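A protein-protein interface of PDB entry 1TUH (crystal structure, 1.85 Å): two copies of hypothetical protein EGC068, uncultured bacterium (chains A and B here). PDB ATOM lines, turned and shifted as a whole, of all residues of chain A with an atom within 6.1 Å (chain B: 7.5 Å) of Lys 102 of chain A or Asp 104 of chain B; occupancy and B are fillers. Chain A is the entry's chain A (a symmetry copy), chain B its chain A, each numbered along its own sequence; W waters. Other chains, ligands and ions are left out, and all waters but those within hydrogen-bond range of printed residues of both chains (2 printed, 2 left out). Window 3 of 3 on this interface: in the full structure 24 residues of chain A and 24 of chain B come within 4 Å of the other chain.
Water W2 bridges the backbone carbonyl oxygen (O) of Val 100 of chain B and the backbone NH (N) of Asp 104 of chain A.
Water W1 lies within hydrogen-bond range of the backbone carbonyl oxygen (O) of Val 100 of chain A (2.8 Å) and the backbone NH (N) of Asp 104 of chain B (3.0 Å).
O of Lys 102 of chain B is in hydrogen-bond range of N of Lys 102 of chain A (2.9 Å).
OD1 of Asp 104 of chain B lies within salt-bridge range of NZ of Lys 102 of chain A (3.1 Å).
The side-chain amino group (NZ) of Lys 102 of chain B is in salt-bridge range of the side-chain carboxylate (OD1) of Asp 104 of chain A, 3.1 Å away.
Ala 28 of chain A touches none of the printed residues of chain B.
Arg 36 of chain A touches none of the printed residues of chain B.
Of the printed residues of chain B, Val 100 of chain A touches Ser 103 (3.7 Å).
Lys 102 of chain A touches three residues of chain B.
Printed residues of chain B within 4 Å of Ile 109 of chain A: Leu 101 (3.5 Å) and Ile 109 (3.5 Å).
Printed residues of chain A within 4 Å of Ser 103 of chain B: Val 100 and Leu 101.
Of chain A, only Lys 102 comes within 4 Å of Asp 104 of chain B.
Of the printed residues of chain A, Ile 109 of chain B touches Leu 101 and Ile 109.
The nearest residue of chain B that does not touch Lys 102 of chain A is Val 100 of chain B (4.4 Å).
Leu 101 of chain B touches its own counterpart, Leu 101 of chain A.
Leu 101 of chain A touches Arg 107 of chain B, and with the chains exchanged Arg 107 of chain A touches Leu 101 of chain B.
Leu 101 of chain A touches Ile 109 of chain B, and with the chains exchanged Ile 109 of chain A touches Leu 101 of chain B.
Lys 102 of chain B touches its own counterpart, Lys 102 of chain A.
Positions printed for both chains: 26, 28, 29, 100, 101, 102, 103, 104, 106, 107 and 109.
Of the 16 pairs that touch across the chains among the printed residues, 15 have their exchanged pair printed and touching as well.
Ser 103 of chain B touches Val 100 of chain A.
O of Leu 101 of chain A touches CD2 of Leu 101 of chain B, at 3.8 Å.
N of Ser 103 of chain B touches CG of Leu 101 of chain A (3.6 Å).
O of Arg 107 of chain B touches CD2 of Leu 101 of chain A, at 3.7 Å.
Leu 101 of chain A touches Ile 109 of chain B.
Ser 103 of chain A touches Val 100 of chain B (CB to O, 3.7 Å).
N of Ser 103 of chain A touches CG of Leu 101 of chain B (3.6 Å).
Arg 107 of chain A touches Leu 101 of chain B (O to CD2, 3.7 Å).
C of Val 108 of chain A touches CD2 of Leu 101 of chain B, at 3.7 Å.
CD2 of Leu 101 of chain B touches N of Ile 109 of chain A, at 3.5 Å.
Of the 14 printed residues of chain A, 8 touch a printed residue of chain B.
Hydrophobic or aromatic side chains of chain B that line the printed part of chain A: Leu 101 and Ile 109.
Among the printed residues, 16 pairs touch across the chains.
Among the printed residues, Asp or Glu carboxylates within 4 Å of a Lys or Arg side-chain nitrogen of the other chain: Lys 102 of chain A with Asp 104 of chain B and Asp 104 of chain A with Lys 102 of chain B.
OG of Ser 103 of chain A sits at hydrogen-bond distance from N of Arg 107 of chain A (3.1 Å).
N of Ile 109 of chain B is in hydrogen-bond range of O of Leu 101 of chain B.
The side-chain carboxylate (OD2) of Asp 105 of chain B is in salt-bridge range of the guanidinium group (NH1) of Arg 107 of chain B (3.6 Å).
OE1 of Glu 29 of chain A is in salt-bridge range of NZ of Lys 102 of chain A (2.6 Å).
The side-chain amino group (NZ) of Lys 102 of chain B lies within salt-bridge range of the side-chain carboxylate (OE1) of Glu 29 of chain B (2.6 Å).
O of Leu 101 of chain A sits at hydrogen-bond distance from N of Ile 109 of chain A, 2.8 Å away.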
ATOM      1  N   ASN A  26     -15.935  24.120   7.818  1.00  0.00           N
ATOM      2  CA  ASN A  26     -15.761  25.606   7.886  1.00  0.00           C
ATOM      3  C   ASN A  26     -14.405  26.080   8.449  1.00  0.00           C
ATOM      4  O   ASN A  26     -13.646  25.308   9.021  1.00  0.00           O
ATOM      5  CB  ASN A  26     -16.966  26.299   8.560  1.00  0.00           C
ATOM      6  CG  ASN A  26     -17.100  26.041  10.085  1.00  0.00           C
ATOM      7  OD1 ASN A  26     -16.191  25.676  10.771  1.00  0.00           O
ATOM      8  ND2 ASN A  26     -18.288  26.311  10.591  1.00  0.00           N
ATOM      9  N   ALA A  28     -13.949  28.049  10.916  1.00  0.00           N
ATOM     10  CA  ALA A  28     -13.918  28.021  12.380  1.00  0.00           C
ATOM     11  C   ALA A  28     -13.538  26.618  12.852  1.00  0.00           C
ATOM     12  O   ALA A  28     -12.723  26.466  13.757  1.00  0.00           O
ATOM     13  CB  ALA A  28     -15.208  28.422  12.956  1.00  0.00           C
ATOM     14  N   GLU A  29     -14.088  25.571  12.230  1.00  0.00           N
ATOM     15  CA  GLU A  29     -13.699  24.238  12.649  1.00  0.00           C
ATOM     16  C   GLU A  29     -12.302  23.851  12.266  1.00  0.00           C
ATOM     17  O   GLU A  29     -11.627  23.160  13.008  1.00  0.00           O
ATOM     18  CB  GLU A  29     -14.731  23.158  12.195  1.00  0.00           C
ATOM     19  CG  GLU A  29     -14.423  21.800  12.801  1.00  0.00           C
ATOM     20  CD  GLU A  29     -14.252  21.776  14.337  1.00  0.00           C
ATOM     21  OE1 GLU A  29     -15.074  22.454  15.058  1.00  0.00           O
ATOM     22  OE2 GLU A  29     -13.310  21.056  14.818  1.00  0.00           O
ATOM     23  N   ALA A  32     -10.274  25.249  14.967  1.00  0.00           N
ATOM     24  CA  ALA A  32     -10.410  24.405  16.139  1.00  0.00           C
ATOM     25  C   ALA A  32      -9.514  23.182  16.025  1.00  0.00           C
ATOM     26  O   ALA A  32      -8.873  22.791  17.007  1.00  0.00           O
ATOM     27  CB  ALA A  32     -11.903  24.046  16.414  1.00  0.00           C
ATOM     28  N   ARG A  36      -6.385  21.950  18.482  1.00  0.00           N
ATOM     29  CA  ARG A  36      -6.207  20.639  19.063  1.00  0.00           C
ATOM     30  C   ARG A  36      -4.846  20.006  18.736  1.00  0.00           C
ATOM     31  O   ARG A  36      -4.209  19.391  19.619  1.00  0.00           O
ATOM     32  CB  ARG A  36      -7.338  19.754  18.632  1.00  0.00           C
ATOM     33  CG  ARG A  36      -8.703  20.184  19.180  1.00  0.00           C
ATOM     34  CD  ARG A  36      -9.796  19.120  18.958  1.00  0.00           C
ATOM     35  NE  ARG A  36     -11.117  19.667  19.226  1.00  0.00           N
ATOM     36  CZ  ARG A  36     -11.922  20.181  18.326  1.00  0.00           C
ATOM     37  NH1 ARG A  36     -11.608  20.298  17.035  1.00  0.00           N
ATOM     38  NH2 ARG A  36     -13.095  20.570  18.735  1.00  0.00           N
ATOM     39  N   VAL A 100     -12.880  22.976  23.651  1.00  0.00           N
ATOM     40  CA  VAL A 100     -12.532  23.879  22.551  1.00  0.00           C
ATOM     41  C   VAL A 100     -13.812  24.587  22.067  1.00  0.00           C
ATOM     42  O   VAL A 100     -14.795  23.953  21.706  1.00  0.00           O
ATOM     43  CB  VAL A 100     -11.833  23.188  21.385  1.00  0.00           C
ATOM     44  CG1 VAL A 100     -11.589  24.167  20.273  1.00  0.00           C
ATOM     45  CG2 VAL A 100     -10.595  22.532  21.804  1.00  0.00           C
ATOM     46  N   LEU A 101     -13.787  25.909  22.099  1.00  0.00           N
ATOM     47  CA  LEU A 101     -14.866  26.742  21.651  1.00  0.00           C
ATOM     48  C   LEU A 101     -14.470  27.613  20.438  1.00  0.00           C
ATOM     49  O   LEU A 101     -13.276  27.955  20.267  1.00  0.00           O
ATOM     50  CB  LEU A 101     -15.430  27.567  22.767  1.00  0.00           C
ATOM     51  CG  LEU A 101     -16.098  26.893  23.985  1.00  0.00           C
ATOM     52  CD1 LEU A 101     -14.990  26.347  24.874  1.00  0.00           C
ATOM     53  CD2 LEU A 101     -16.993  27.883  24.767  1.00  0.00           C
ATOM     54  N   LYS A 102     -15.467  27.984  19.624  1.00  0.00           N
ATOM     55  CA  LYS A 102     -15.267  28.691  18.347  1.00  0.00           C
ATOM     56  C   LYS A 102     -16.227  29.810  18.223  1.00  0.00           C
ATOM     57  O   LYS A 102     -17.428  29.681  18.568  1.00  0.00           O
ATOM     58  CB  LYS A 102     -15.633  27.779  17.112  1.00  0.00           C
ATOM     59  CG  LYS A 102     -14.875  26.570  16.974  1.00  0.00           C
ATOM     60  CD  LYS A 102     -15.520  25.628  15.894  1.00  0.00           C
ATOM     61  CE  LYS A 102     -16.637  24.737  16.464  1.00  0.00           C
ATOM     62  NZ  LYS A 102     -17.199  23.901  15.366  1.00  0.00           N
ATOM     63  N   SER A 103     -15.788  30.888  17.598  1.00  0.00           N
ATOM     64  CA  SER A 103     -16.717  31.875  17.142  1.00  0.00           C
ATOM     65  C   SER A 103     -16.958  31.582  15.665  1.00  0.00           C
ATOM     66  O   SER A 103     -16.163  30.906  14.974  1.00  0.00           O
ATOM     67  CB  SER A 103     -16.211  33.305  17.322  1.00  0.00           C
ATOM     68  OG  SER A 103     -15.042  33.513  16.555  1.00  0.00           O
ATOM     69  N   ASP A 104     -18.026  32.167  15.170  1.00  0.00           N
ATOM     70  CA  ASP A 104     -18.437  31.896  13.814  1.00  0.00           C
ATOM     71  C   ASP A 104     -17.332  32.414  12.937  1.00  0.00           C
ATOM     72  O   ASP A 104     -17.073  31.809  11.892  1.00  0.00           O
ATOM     73  CB  ASP A 104     -19.808  32.560  13.464  1.00  0.00           C
ATOM     74  CG  ASP A 104     -20.996  31.963  14.308  1.00  0.00           C
ATOM     75  OD1 ASP A 104     -20.950  30.741  14.720  1.00  0.00           O
ATOM     76  OD2 ASP A 104     -22.032  32.623  14.587  1.00  0.00           O
ATOM     77  N   GLY A 106     -14.035  32.300  13.381  1.00  0.00           N
ATOM     78  CA  GLY A 106     -12.787  31.553  13.453  1.00  0.00           C
ATOM     79  C   GLY A 106     -11.841  31.802  14.650  1.00  0.00           C
ATOM     80  O   GLY A 106     -10.775  31.188  14.693  1.00  0.00           O
ATOM     81  N   ARG A 107     -12.201  32.719  15.568  1.00  0.00           N
ATOM     82  CA  ARG A 107     -11.533  32.790  16.883  1.00  0.00           C
ATOM     83  C   ARG A 107     -11.783  31.464  17.561  1.00  0.00           C
ATOM     84  O   ARG A 107     -12.881  30.883  17.419  1.00  0.00           O
ATOM     85  CB  ARG A 107     -12.147  33.862  17.756  1.00  0.00           C
ATOM     86  CG  ARG A 107     -11.249  34.851  18.393  1.00  0.00           C
ATOM     87  CD  ARG A 107     -11.930  36.277  18.684  1.00  0.00           C
ATOM     88  NE  ARG A 107     -11.073  37.452  18.410  1.00  0.00           N
ATOM     89  CZ  ARG A 107     -11.191  38.271  17.370  1.00  0.00           C
ATOM     90  NH1 ARG A 107     -12.142  38.108  16.452  1.00  0.00           N
ATOM     91  NH2 ARG A 107     -10.375  39.292  17.260  1.00  0.00           N
ATOM     92  N   VAL A 108     -10.833  31.023  18.388  1.00  0.00           N
ATOM     93  CA  VAL A 108     -10.962  29.751  19.108  1.00  0.00           C
ATOM     94  C   VAL A 108     -10.501  29.984  20.536  1.00  0.00           C
ATOM     95  O   VAL A 108      -9.548  30.750  20.742  1.00  0.00           O
ATOM     96  CB  VAL A 108     -10.104  28.668  18.482  1.00  0.00           C
ATOM     97  CG1 VAL A 108     -10.159  27.325  19.235  1.00  0.00           C
ATOM     98  CG2 VAL A 108     -10.511  28.410  17.009  1.00  0.00           C
ATOM     99  N   ILE A 109     -11.179  29.375  21.491  1.00  0.00           N
ATOM    100  CA  ILE A 109     -10.622  29.252  22.847  1.00  0.00           C
ATOM    101  C   ILE A 109     -10.381  27.785  23.181  1.00  0.00           C
ATOM    102  O   ILE A 109     -11.242  26.909  22.942  1.00  0.00           O
ATOM    103  CB  ILE A 109     -11.544  29.905  23.877  1.00  0.00           C
ATOM    104  CG1 ILE A 109     -11.442  31.413  23.740  1.00  0.00           C
ATOM    105  CG2 ILE A 109     -11.233  29.476  25.329  1.00  0.00           C
ATOM    106  CD1 ILE A 109     -12.534  32.194  24.544  1.00  0.00           C
ATOM    107  N   ASN B  26     -29.476  25.523  16.403  1.00  0.00           N
ATOM    108  CA  ASN B  26     -28.941  24.516  17.374  1.00  0.00           C
ATOM    109  C   ASN B  26     -28.910  24.979  18.846  1.00  0.00           C
ATOM    110  O   ASN B  26     -29.073  26.154  19.148  1.00  0.00           O
ATOM    111  CB  ASN B  26     -27.597  23.917  16.904  1.00  0.00           C
ATOM    112  CG  ASN B  26     -26.394  24.897  16.947  1.00  0.00           C
ATOM    113  OD1 ASN B  26     -26.379  25.887  17.619  1.00  0.00           O
ATOM    114  ND2 ASN B  26     -25.352  24.529  16.228  1.00  0.00           N
ATOM    115  N   GLU B  27     -28.754  24.013  19.733  1.00  0.00           N
ATOM    116  CA  GLU B  27     -28.622  24.252  21.143  1.00  0.00           C
ATOM    117  C   GLU B  27     -27.511  25.254  21.408  1.00  0.00           C
ATOM    118  O   GLU B  27     -27.689  26.182  22.208  1.00  0.00           O
ATOM    119  CB  GLU B  27     -28.249  22.946  21.868  1.00  0.00           C
ATOM    120  CG  GLU B  27     -28.036  23.072  23.376  1.00  0.00           C
ATOM    121  CD  GLU B  27     -27.633  21.734  24.060  1.00  0.00           C
ATOM    122  OE1 GLU B  27     -26.728  20.987  23.591  1.00  0.00           O
ATOM    123  OE2 GLU B  27     -28.270  21.421  25.090  1.00  0.00           O
ATOM    124  N   ALA B  28     -26.371  25.034  20.773  1.00  0.00           N
ATOM    125  CA  ALA B  28     -25.205  25.870  21.065  1.00  0.00           C
ATOM    126  C   ALA B  28     -25.515  27.320  20.694  1.00  0.00           C
ATOM    127  O   ALA B  28     -25.200  28.237  21.447  1.00  0.00           O
ATOM    128  CB  ALA B  28     -24.011  25.405  20.347  1.00  0.00           C
ATOM    129  N   GLU B  29     -26.168  27.555  19.552  1.00  0.00           N
ATOM    130  CA  GLU B  29     -26.500  28.926  19.216  1.00  0.00           C
ATOM    131  C   GLU B  29     -27.579  29.529  20.066  1.00  0.00           C
ATOM    132  O   GLU B  29     -27.535  30.705  20.378  1.00  0.00           O
ATOM    133  CB  GLU B  29     -26.814  29.097  17.697  1.00  0.00           C
ATOM    134  CG  GLU B  29     -26.967  30.560  17.317  1.00  0.00           C
ATOM    135  CD  GLU B  29     -25.803  31.486  17.740  1.00  0.00           C
ATOM    136  OE1 GLU B  29     -24.597  31.067  17.583  1.00  0.00           O
ATOM    137  OE2 GLU B  29     -26.101  32.640  18.203  1.00  0.00           O
ATOM    138  N   VAL B 100     -18.392  36.219  21.309  1.00  0.00           N
ATOM    139  CA  VAL B 100     -19.104  35.071  21.876  1.00  0.00           C
ATOM    140  C   VAL B 100     -18.662  33.797  21.131  1.00  0.00           C
ATOM    141  O   VAL B 100     -18.755  33.704  19.913  1.00  0.00           O
ATOM    142  CB  VAL B 100     -20.621  35.209  21.840  1.00  0.00           C
ATOM    143  CG1 VAL B 100     -21.268  33.958  22.362  1.00  0.00           C
ATOM    144  CG2 VAL B 100     -21.078  36.392  22.567  1.00  0.00           C
ATOM    145  N   LEU B 101     -18.151  32.836  21.884  1.00  0.00           N
ATOM    146  CA  LEU B 101     -17.723  31.564  21.378  1.00  0.00           C
ATOM    147  C   LEU B 101     -18.559  30.395  21.945  1.00  0.00           C
ATOM    148  O   LEU B 101     -19.102  30.494  23.070  1.00  0.00           O
ATOM    149  CB  LEU B 101     -16.255  31.349  21.587  1.00  0.00           C
ATOM    150  CG  LEU B 101     -15.220  32.272  20.908  1.00  0.00           C
ATOM    151  CD1 LEU B 101     -15.195  33.583  21.681  1.00  0.00           C
ATOM    152  CD2 LEU B 101     -13.815  31.627  20.875  1.00  0.00           C
ATOM    153  N   LYS B 102     -18.638  29.298  21.181  1.00  0.00           N
ATOM    154  CA  LYS B 102     -19.501  28.143  21.485  1.00  0.00           C
ATOM    155  C   LYS B 102     -18.754  26.880  21.296  1.00  0.00           C
ATOM    156  O   LYS B 102     -17.987  26.715  20.315  1.00  0.00           O
ATOM    157  CB  LYS B 102     -20.683  28.009  20.449  1.00  0.00           C
ATOM    158  CG  LYS B 102     -21.586  29.119  20.375  1.00  0.00           C
ATOM    159  CD  LYS B 102     -22.529  28.988  19.124  1.00  0.00           C
ATOM    160  CE  LYS B 102     -21.902  29.548  17.837  1.00  0.00           C
ATOM    161  NZ  LYS B 102     -22.857  29.360  16.709  1.00  0.00           N
ATOM    162  N   SER B 103     -19.055  25.895  22.125  1.00  0.00           N
ATOM    163  CA  SER B 103     -18.642  24.559  21.823  1.00  0.00           C
ATOM    164  C   SER B 103     -19.845  23.877  21.182  1.00  0.00           C
ATOM    165  O   SER B 103     -21.014  24.300  21.324  1.00  0.00           O
ATOM    166  CB  SER B 103     -18.185  23.780  23.056  1.00  0.00           C
ATOM    167  OG  SER B 103     -19.252  23.641  23.972  1.00  0.00           O
ATOM    168  N   ASP B 104     -19.552  22.768  20.540  1.00  0.00           N
ATOM    169  CA  ASP B 104     -20.574  22.071  19.796  1.00  0.00           C
ATOM    170  C   ASP B 104     -21.584  21.617  20.810  1.00  0.00           C
ATOM    171  O   ASP B 104     -22.777  21.592  20.486  1.00  0.00           O
ATOM    172  CB  ASP B 104     -19.998  20.870  18.979  1.00  0.00           C
ATOM    173  CG  ASP B 104     -19.006  21.334  17.846  1.00  0.00           C
ATOM    174  OD1 ASP B 104     -19.149  22.491  17.292  1.00  0.00           O
ATOM    175  OD2 ASP B 104     -18.070  20.607  17.421  1.00  0.00           O
ATOM    176  N   ASP B 105     -21.113  21.278  22.028  1.00  0.00           N
ATOM    177  CA  ASP B 105     -21.975  20.829  23.132  1.00  0.00           C
ATOM    178  C   ASP B 105     -22.743  21.930  23.970  1.00  0.00           C
ATOM    179  O   ASP B 105     -23.369  21.599  24.980  1.00  0.00           O
ATOM    180  CB  ASP B 105     -21.197  19.886  24.077  1.00  0.00           C
ATOM    181  CG  ASP B 105     -20.116  20.601  24.904  1.00  0.00           C
ATOM    182  OD1 ASP B 105     -20.025  21.852  25.005  1.00  0.00           O
ATOM    183  OD2 ASP B 105     -19.252  19.925  25.502  1.00  0.00           O
ATOM    184  N   GLY B 106     -22.736  23.181  23.513  1.00  0.00           N
ATOM    185  CA  GLY B 106     -23.513  24.245  24.131  1.00  0.00           C
ATOM    186  C   GLY B 106     -22.868  25.071  25.268  1.00  0.00           C
ATOM    187  O   GLY B 106     -23.538  25.953  25.806  1.00  0.00           O
ATOM    188  N   ARG B 107     -21.618  24.756  25.655  1.00  0.00           N
ATOM    189  CA  ARG B 107     -20.820  25.675  26.492  1.00  0.00           C
ATOM    190  C   ARG B 107     -20.654  26.945  25.691  1.00  0.00           C
ATOM    191  O   ARG B 107     -20.498  26.890  24.451  1.00  0.00           O
ATOM    192  CB  ARG B 107     -19.435  25.124  26.749  1.00  0.00           C
ATOM    193  CG  ARG B 107     -18.947  25.071  28.145  1.00  0.00           C
ATOM    194  CD  ARG B 107     -17.873  23.911  28.431  1.00  0.00           C
ATOM    195  NE  ARG B 107     -18.037  23.204  29.721  1.00  0.00           N
ATOM    196  CZ  ARG B 107     -18.524  21.977  29.874  1.00  0.00           C
ATOM    197  NH1 ARG B 107     -18.907  21.238  28.835  1.00  0.00           N
ATOM    198  NH2 ARG B 107     -18.595  21.459  31.078  1.00  0.00           N
ATOM    199  N   ILE B 109     -18.510  30.890  25.791  1.00  0.00           N
ATOM    200  CA  ILE B 109     -17.702  31.935  26.438  1.00  0.00           C
ATOM    201  C   ILE B 109     -18.087  33.305  25.892  1.00  0.00           C
ATOM    202  O   ILE B 109     -18.226  33.506  24.664  1.00  0.00           O
ATOM    203  CB  ILE B 109     -16.209  31.668  26.245  1.00  0.00           C
ATOM    204  CG1 ILE B 109     -15.801  30.505  27.130  1.00  0.00           C
ATOM    205  CG2 ILE B 109     -15.327  32.903  26.542  1.00  0.00           C
ATOM    206  CD1 ILE B 109     -14.368  29.954  26.826  1.00  0.00           C
HETATM  207  O   HOH W   1     -16.600  22.606  20.032  1.00  0.00           O
HETATM  208  O   HOH W   2     -19.816  33.115  17.384  1.00  0.00           O
